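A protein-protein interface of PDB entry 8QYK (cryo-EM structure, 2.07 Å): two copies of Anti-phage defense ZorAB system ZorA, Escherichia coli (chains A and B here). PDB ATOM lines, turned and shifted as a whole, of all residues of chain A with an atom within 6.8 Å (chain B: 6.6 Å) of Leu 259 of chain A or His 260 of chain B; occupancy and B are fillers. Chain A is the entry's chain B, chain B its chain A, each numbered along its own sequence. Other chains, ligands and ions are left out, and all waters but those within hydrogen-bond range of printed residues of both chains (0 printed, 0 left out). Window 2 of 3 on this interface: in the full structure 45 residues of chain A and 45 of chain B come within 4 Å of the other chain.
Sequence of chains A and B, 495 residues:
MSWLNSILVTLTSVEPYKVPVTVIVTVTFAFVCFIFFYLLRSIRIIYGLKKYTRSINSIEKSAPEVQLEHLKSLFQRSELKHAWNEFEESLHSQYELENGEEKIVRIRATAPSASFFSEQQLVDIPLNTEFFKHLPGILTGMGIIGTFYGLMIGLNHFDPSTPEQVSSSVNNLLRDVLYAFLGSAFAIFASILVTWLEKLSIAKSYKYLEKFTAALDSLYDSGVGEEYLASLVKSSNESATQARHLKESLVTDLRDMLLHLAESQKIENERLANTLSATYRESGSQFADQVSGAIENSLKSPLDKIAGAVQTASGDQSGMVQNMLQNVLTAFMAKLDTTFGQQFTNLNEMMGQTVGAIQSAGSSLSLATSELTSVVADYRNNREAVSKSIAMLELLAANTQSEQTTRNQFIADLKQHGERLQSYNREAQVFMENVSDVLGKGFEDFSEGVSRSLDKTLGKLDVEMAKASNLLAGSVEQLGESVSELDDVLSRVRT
O of His 260 of chain B lies within hydrogen-bond range of OG of Ser 264 of chain B.
Among the printed residues, merely in contact across the chains: Leu 254 of chain A with Met 257 of chain B, Arg 255 of chain A with Met 257 of chain B, Leu 258 of chain A with Met 257 of chain B, Leu 258 of chain A with Leu 258 of chain B and Leu 259 of chain A with His 260 of chain B.
Printed residues of chain B within 4 Å of Leu 259 of chain A: His 260 (3.95 Å). His 260 of chain B touches one residue of chain A. Of the printed residues of chain A, Met 257 of chain B touches Leu 254 (3.1 Å), Arg 255 (3.4 Å) and Leu 258 (3.5 Å). Of the printed residues of chain A, Leu 258 of chain B touches Leu 258. Printed residues of chain B within 4 Å of Arg 255 of chain A: Met 257. Glu 263 of chain B touches none of the printed residues of chain A. Ala 262 of chain B touches none of the printed residues of chain A. The nearest residue of chain A that does not touch His 260 of chain B is Ala 262 of chain A (5.8 Å).
Hydrophobic or aromatic side chains of chain A within 4 Å of the printed part of chain B: Leu 254, Leu 258 and Leu 259. Along chain A the printed residues that touch a printed residue of chain B span positions 254 to 259. Of the 11 printed residues of chain B, 3 touch a printed residue of chain A. Printed residues of chain B that touch a printed residue of chain A: Met 257, Leu 258 and His 260. Hydrophobic or aromatic side chains of chain B that line the printed part of chain A: Met 257, Leu 258 and His 260. Among the printed residues, 5 pairs touch across the chains. Among the printed residues, no Asp or Glu carboxylate lies within 4 Å of a Lys or Arg side-chain nitrogen of the other chain.
Arg 255 of chain A touches Met 257 of chain B, but with the chains exchanged Met 257 of chain A does not touch Arg 255 of chain B (13.4 Å). Leu 258 of chain A touches Met 257 of chain B, but with the chains exchanged Met 257 of chain A does not touch Leu 258 of chain B (9.3 Å). Leu 258 of chain B touches its own counterpart, Leu 258 of chain A. Leu 259 of chain A touches His 260 of chain B, but with the chains exchanged His 260 of chain A does not touch Leu 259 of chain B (13.4 Å). Positions printed for both chains: 255, 256, 257, 258, 259, 260, 261, 262, 263 and 264.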
ATOM      1  N   LEU A 254     -16.012  18.502  24.728  1.00  0.00           N
ATOM      2  CA  LEU A 254     -16.802  19.495  24.010  1.00  0.00           C
ATOM      3  C   LEU A 254     -17.859  20.113  24.913  1.00  0.00           C
ATOM      4  O   LEU A 254     -18.089  21.329  24.872  1.00  0.00           O
ATOM      5  CB  LEU A 254     -17.459  18.859  22.784  1.00  0.00           C
ATOM      6  CG  LEU A 254     -16.599  18.517  21.569  1.00  0.00           C
ATOM      7  CD1 LEU A 254     -17.427  17.750  20.550  1.00  0.00           C
ATOM      8  CD2 LEU A 254     -16.020  19.770  20.945  1.00  0.00           C
ATOM      9  N   ARG A 255     -18.539  19.287  25.714  1.00  0.00           N
ATOM     10  CA  ARG A 255     -19.553  19.806  26.625  1.00  0.00           C
ATOM     11  C   ARG A 255     -18.935  20.777  27.619  1.00  0.00           C
ATOM     12  O   ARG A 255     -19.496  21.845  27.896  1.00  0.00           O
ATOM     13  CB  ARG A 255     -20.251  18.658  27.356  1.00  0.00           C
ATOM     14  CG  ARG A 255     -21.610  18.277  26.788  1.00  0.00           C
ATOM     15  CD  ARG A 255     -22.283  17.217  27.650  1.00  0.00           C
ATOM     16  NE  ARG A 255     -23.655  16.951  27.232  1.00  0.00           N
ATOM     17  CZ  ARG A 255     -24.006  16.075  26.301  1.00  0.00           C
ATOM     18  NH1 ARG A 255     -23.107  15.349  25.659  1.00  0.00           N
ATOM     19  NH2 ARG A 255     -25.295  15.926  26.003  1.00  0.00           N
ATOM     20  N   ASP A 256     -17.767  20.423  28.158  1.00  0.00           N
ATOM     21  CA  ASP A 256     -17.083  21.317  29.087  1.00  0.00           C
ATOM     22  C   ASP A 256     -16.714  22.636  28.415  1.00  0.00           C
ATOM     23  O   ASP A 256     -16.913  23.714  28.993  1.00  0.00           O
ATOM     24  CB  ASP A 256     -15.838  20.635  29.649  1.00  0.00           C
ATOM     25  CG  ASP A 256     -14.938  21.595  30.399  1.00  0.00           C
ATOM     26  OD1 ASP A 256     -15.309  22.011  31.516  1.00  0.00           O
ATOM     27  OD2 ASP A 256     -13.861  21.936  29.866  1.00  0.00           O
ATOM     28  N   MET A 257     -16.176  22.571  27.193  1.00  0.00           N
ATOM     29  CA  MET A 257     -15.779  23.793  26.498  1.00  0.00           C
ATOM     30  C   MET A 257     -16.979  24.684  26.199  1.00  0.00           C
ATOM     31  O   MET A 257     -16.905  25.906  26.363  1.00  0.00           O
ATOM     32  CB  MET A 257     -15.021  23.457  25.213  1.00  0.00           C
ATOM     33  CG  MET A 257     -13.674  22.793  25.449  1.00  0.00           C
ATOM     34  SD  MET A 257     -12.753  22.459  23.935  1.00  0.00           S
ATOM     35  CE  MET A 257     -13.661  21.067  23.278  1.00  0.00           C
ATOM     36  N   LEU A 258     -18.098  24.097  25.764  1.00  0.00           N
ATOM     37  CA  LEU A 258     -19.273  24.919  25.484  1.00  0.00           C
ATOM     38  C   LEU A 258     -19.893  25.484  26.755  1.00  0.00           C
ATOM     39  O   LEU A 258     -20.396  26.613  26.741  1.00  0.00           O
ATOM     40  CB  LEU A 258     -20.311  24.135  24.683  1.00  0.00           C
ATOM     41  CG  LEU A 258     -19.984  23.956  23.199  1.00  0.00           C
ATOM     42  CD1 LEU A 258     -21.242  23.639  22.409  1.00  0.00           C
ATOM     43  CD2 LEU A 258     -19.305  25.196  22.642  1.00  0.00           C
ATOM     44  N   LEU A 259     -19.874  24.734  27.861  1.00  0.00           N
ATOM     45  CA  LEU A 259     -20.350  25.292  29.124  1.00  0.00           C
ATOM     46  C   LEU A 259     -19.490  26.474  29.556  1.00  0.00           C
ATOM     47  O   LEU A 259     -20.013  27.514  29.985  1.00  0.00           O
ATOM     48  CB  LEU A 259     -20.364  24.209  30.203  1.00  0.00           C
ATOM     49  CG  LEU A 259     -21.500  23.189  30.115  1.00  0.00           C
ATOM     50  CD1 LEU A 259     -21.470  22.246  31.309  1.00  0.00           C
ATOM     51  CD2 LEU A 259     -22.845  23.889  30.014  1.00  0.00           C
ATOM     52  N   HIS A 260     -18.167  26.340  29.434  1.00  0.00           N
ATOM     53  CA  HIS A 260     -17.279  27.449  29.767  1.00  0.00           C
ATOM     54  C   HIS A 260     -17.521  28.645  28.852  1.00  0.00           C
ATOM     55  O   HIS A 260     -17.501  29.795  29.304  1.00  0.00           O
ATOM     56  CB  HIS A 260     -15.821  26.997  29.690  1.00  0.00           C
ATOM     57  CG  HIS A 260     -15.319  26.369  30.953  1.00  0.00           C
ATOM     58  ND1 HIS A 260     -14.751  27.101  31.973  1.00  0.00           N
ATOM     59  CD2 HIS A 260     -15.305  25.079  31.363  1.00  0.00           C
ATOM     60  CE1 HIS A 260     -14.406  26.290  32.956  1.00  0.00           C
ATOM     61  NE2 HIS A 260     -14.732  25.057  32.612  1.00  0.00           N
ATOM     62  N   LEU A 261     -17.745  28.392  27.559  1.00  0.00           N
ATOM     63  CA  LEU A 261     -18.025  29.480  26.627  1.00  0.00           C
ATOM     64  C   LEU A 261     -19.323  30.195  26.981  1.00  0.00           C
ATOM     65  O   LEU A 261     -19.402  31.425  26.908  1.00  0.00           O
ATOM     66  CB  LEU A 261     -18.084  28.947  25.196  1.00  0.00           C
ATOM     67  CG  LEU A 261     -18.415  29.985  24.122  1.00  0.00           C
ATOM     68  CD1 LEU A 261     -17.200  30.846  23.814  1.00  0.00           C
ATOM     69  CD2 LEU A 261     -18.948  29.320  22.864  1.00  0.00           C
ATOM     70  N   ALA A 262     -20.357  29.437  27.352  1.00  0.00           N
ATOM     71  CA  ALA A 262     -21.619  30.050  27.754  1.00  0.00           C
ATOM     72  C   ALA A 262     -21.443  30.898  29.007  1.00  0.00           C
ATOM     73  O   ALA A 262     -21.993  32.002  29.100  1.00  0.00           O
ATOM     74  CB  ALA A 262     -22.681  28.974  27.975  1.00  0.00           C
ATOM     75  N   GLU A 263     -20.678  30.399  29.982  1.00  0.00           N
ATOM     76  CA  GLU A 263     -20.417  31.187  31.184  1.00  0.00           C
ATOM     77  C   GLU A 263     -19.651  32.464  30.856  1.00  0.00           C
ATOM     78  O   GLU A 263     -19.955  33.540  31.393  1.00  0.00           O
ATOM     79  CB  GLU A 263     -19.653  30.347  32.207  1.00  0.00           C
ATOM     80  CG  GLU A 263     -20.504  29.293  32.889  1.00  0.00           C
ATOM     81  CD  GLU A 263     -21.587  29.902  33.759  1.00  0.00           C
ATOM     82  OE1 GLU A 263     -21.331  30.959  34.375  1.00  0.00           O
ATOM     83  OE2 GLU A 263     -22.694  29.328  33.822  1.00  0.00           O
ATOM     84  N   SER A 264     -18.653  32.366  29.974  1.00  0.00           N
ATOM     85  CA  SER A 264     -17.895  33.547  29.575  1.00  0.00           C
ATOM     86  C   SER A 264     -18.784  34.557  28.865  1.00  0.00           C
ATOM     87  O   SER A 264     -18.669  35.765  29.095  1.00  0.00           O
ATOM     88  CB  SER A 264     -16.724  33.142  28.679  1.00  0.00           C
ATOM     89  OG  SER A 264     -17.185  32.595  27.455  1.00  0.00           O
ATOM     90  N   ARG B 255     -25.611  18.475  17.764  1.00  0.00           N
ATOM     91  CA  ARG B 255     -26.905  19.142  17.644  1.00  0.00           C
ATOM     92  C   ARG B 255     -27.464  19.504  19.013  1.00  0.00           C
ATOM     93  O   ARG B 255     -27.903  20.641  19.236  1.00  0.00           O
ATOM     94  CB  ARG B 255     -27.895  18.254  16.890  1.00  0.00           C
ATOM     95  CG  ARG B 255     -27.525  17.997  15.448  1.00  0.00           C
ATOM     96  CD  ARG B 255     -28.604  17.228  14.712  1.00  0.00           C
ATOM     97  NE  ARG B 255     -28.211  16.951  13.336  1.00  0.00           N
ATOM     98  CZ  ARG B 255     -28.176  17.861  12.372  1.00  0.00           C
ATOM     99  NH1 ARG B 255     -28.507  19.122  12.599  1.00  0.00           N
ATOM    100  NH2 ARG B 255     -27.798  17.497  11.150  1.00  0.00           N
ATOM    101  N   ASP B 256     -27.447  18.549  19.946  1.00  0.00           N
ATOM    102  CA  ASP B 256     -27.958  18.818  21.287  1.00  0.00           C
ATOM    103  C   ASP B 256     -27.173  19.940  21.956  1.00  0.00           C
ATOM    104  O   ASP B 256     -27.755  20.837  22.582  1.00  0.00           O
ATOM    105  CB  ASP B 256     -27.912  17.541  22.128  1.00  0.00           C
ATOM    106  CG  ASP B 256     -28.795  17.615  23.362  1.00  0.00           C
ATOM    107  OD1 ASP B 256     -28.737  18.632  24.084  1.00  0.00           O
ATOM    108  OD2 ASP B 256     -29.548  16.652  23.614  1.00  0.00           O
ATOM    109  N   MET B 257     -25.847  19.917  21.812  1.00  0.00           N
ATOM    110  CA  MET B 257     -24.999  20.932  22.426  1.00  0.00           C
ATOM    111  C   MET B 257     -25.297  22.321  21.879  1.00  0.00           C
ATOM    112  O   MET B 257     -25.392  23.291  22.642  1.00  0.00           O
ATOM    113  CB  MET B 257     -23.537  20.580  22.182  1.00  0.00           C
ATOM    114  CG  MET B 257     -23.071  19.328  22.881  1.00  0.00           C
ATOM    115  SD  MET B 257     -21.369  19.008  22.423  1.00  0.00           S
ATOM    116  CE  MET B 257     -20.618  20.352  23.300  1.00  0.00           C
ATOM    117  N   LEU B 258     -25.432  22.447  20.558  1.00  0.00           N
ATOM    118  CA  LEU B 258     -25.624  23.779  19.999  1.00  0.00           C
ATOM    119  C   LEU B 258     -27.042  24.284  20.245  1.00  0.00           C
ATOM    120  O   LEU B 258     -27.255  25.493  20.373  1.00  0.00           O
ATOM    121  CB  LEU B 258     -25.267  23.803  18.515  1.00  0.00           C
ATOM    122  CG  LEU B 258     -23.753  23.930  18.300  1.00  0.00           C
ATOM    123  CD1 LEU B 258     -23.420  24.322  16.875  1.00  0.00           C
ATOM    124  CD2 LEU B 258     -23.137  24.918  19.281  1.00  0.00           C
ATOM    125  N   LEU B 259     -28.019  23.378  20.350  1.00  0.00           N
ATOM    126  CA  LEU B 259     -29.341  23.801  20.809  1.00  0.00           C
ATOM    127  C   LEU B 259     -29.294  24.297  22.251  1.00  0.00           C
ATOM    128  O   LEU B 259     -29.958  25.282  22.598  1.00  0.00           O
ATOM    129  CB  LEU B 259     -30.351  22.665  20.659  1.00  0.00           C
ATOM    130  CG  LEU B 259     -31.171  22.666  19.364  1.00  0.00           C
ATOM    131  CD1 LEU B 259     -30.343  22.276  18.146  1.00  0.00           C
ATOM    132  CD2 LEU B 259     -32.391  21.765  19.504  1.00  0.00           C
ATOM    133  N   HIS B 260     -28.517  23.628  23.107  1.00  0.00           N
ATOM    134  CA  HIS B 260     -28.337  24.117  24.473  1.00  0.00           C
ATOM    135  C   HIS B 260     -27.693  25.501  24.480  1.00  0.00           C
ATOM    136  O   HIS B 260     -28.104  26.387  25.242  1.00  0.00           O
ATOM    137  CB  HIS B 260     -27.493  23.122  25.272  1.00  0.00           C
ATOM    138  CG  HIS B 260     -27.316  23.493  26.711  1.00  0.00           C
ATOM    139  ND1 HIS B 260     -26.349  24.376  27.140  1.00  0.00           N
ATOM    140  CD2 HIS B 260     -27.977  23.090  27.823  1.00  0.00           C
ATOM    141  CE1 HIS B 260     -26.424  24.505  28.453  1.00  0.00           C
ATOM    142  NE2 HIS B 260     -27.404  23.736  28.891  1.00  0.00           N
ATOM    143  N   LEU B 261     -26.681  25.703  23.632  1.00  0.00           N
ATOM    144  CA  LEU B 261     -26.031  27.008  23.543  1.00  0.00           C
ATOM    145  C   LEU B 261     -27.002  28.076  23.050  1.00  0.00           C
ATOM    146  O   LEU B 261     -26.979  29.217  23.529  1.00  0.00           O
ATOM    147  CB  LEU B 261     -24.810  26.925  22.626  1.00  0.00           C
ATOM    148  CG  LEU B 261     -23.943  28.180  22.520  1.00  0.00           C
ATOM    149  CD1 LEU B 261     -22.933  28.234  23.657  1.00  0.00           C
ATOM    150  CD2 LEU B 261     -23.241  28.242  21.172  1.00  0.00           C
ATOM    151  N   ALA B 262     -27.860  27.728  22.088  1.00  0.00           N
ATOM    152  CA  ALA B 262     -28.858  28.674  21.601  1.00  0.00           C
ATOM    153  C   ALA B 262     -29.867  29.026  22.688  1.00  0.00           C
ATOM    154  O   ALA B 262     -30.289  30.182  22.801  1.00  0.00           O
ATOM    155  CB  ALA B 262     -29.568  28.106  20.373  1.00  0.00           C
ATOM    156  N   GLU B 263     -30.278  28.040  23.489  1.00  0.00           N
ATOM    157  CA  GLU B 263     -31.181  28.326  24.601  1.00  0.00           C
ATOM    158  C   GLU B 263     -30.518  29.245  25.622  1.00  0.00           C
ATOM    159  O   GLU B 263     -31.158  30.157  26.164  1.00  0.00           O
ATOM    160  CB  GLU B 263     -31.637  27.023  25.261  1.00  0.00           C
ATOM    161  CG  GLU B 263     -32.469  27.223  26.519  1.00  0.00           C
ATOM    162  CD  GLU B 263     -32.816  25.915  27.208  1.00  0.00           C
ATOM    163  OE1 GLU B 263     -32.341  24.854  26.751  1.00  0.00           O
ATOM    164  OE2 GLU B 263     -33.565  25.948  28.207  1.00  0.00           O
ATOM    165  N   SER B 264     -29.231  29.017  25.897  1.00  0.00           N
ATOM    166  CA  SER B 264     -28.500  29.906  26.796  1.00  0.00           C
ATOM    167  C   SER B 264     -28.430  31.321  26.232  1.00  0.00           C
ATOM    168  O   SER B 264     -28.584  32.303  26.970  1.00  0.00           O
ATOM    169  CB  SER B 264     -27.096  29.359  27.046  1.00  0.00           C
ATOM    170  OG  SER B 264     -27.150  28.075  27.642  1.00  0.00           O
ATOM    171  N   GLN B 265     -28.194  31.443  24.924  1.00  0.00           N
ATOM    172  CA  GLN B 265     -28.175  32.759  24.290  1.00  0.00           C
ATOM    173  C   GLN B 265     -29.539  33.432  24.377  1.00  0.00           C
ATOM    174  O   GLN B 265     -29.626  34.652  24.551  1.00  0.00           O
ATOM    175  CB  GLN B 265     -27.726  32.634  22.834  1.00  0.00           C
ATOM    176  CG  GLN B 265     -27.638  33.960  22.095  1.00  0.00           C
ATOM    177  CD  GLN B 265     -26.648  34.917  22.731  1.00  0.00           C
ATOM    178  OE1 GLN B 265     -27.038  35.884  23.388  1.00  0.00           O
ATOM    179  NE2 GLN B 265     -25.360  34.652  22.541  1.00  0.00           N
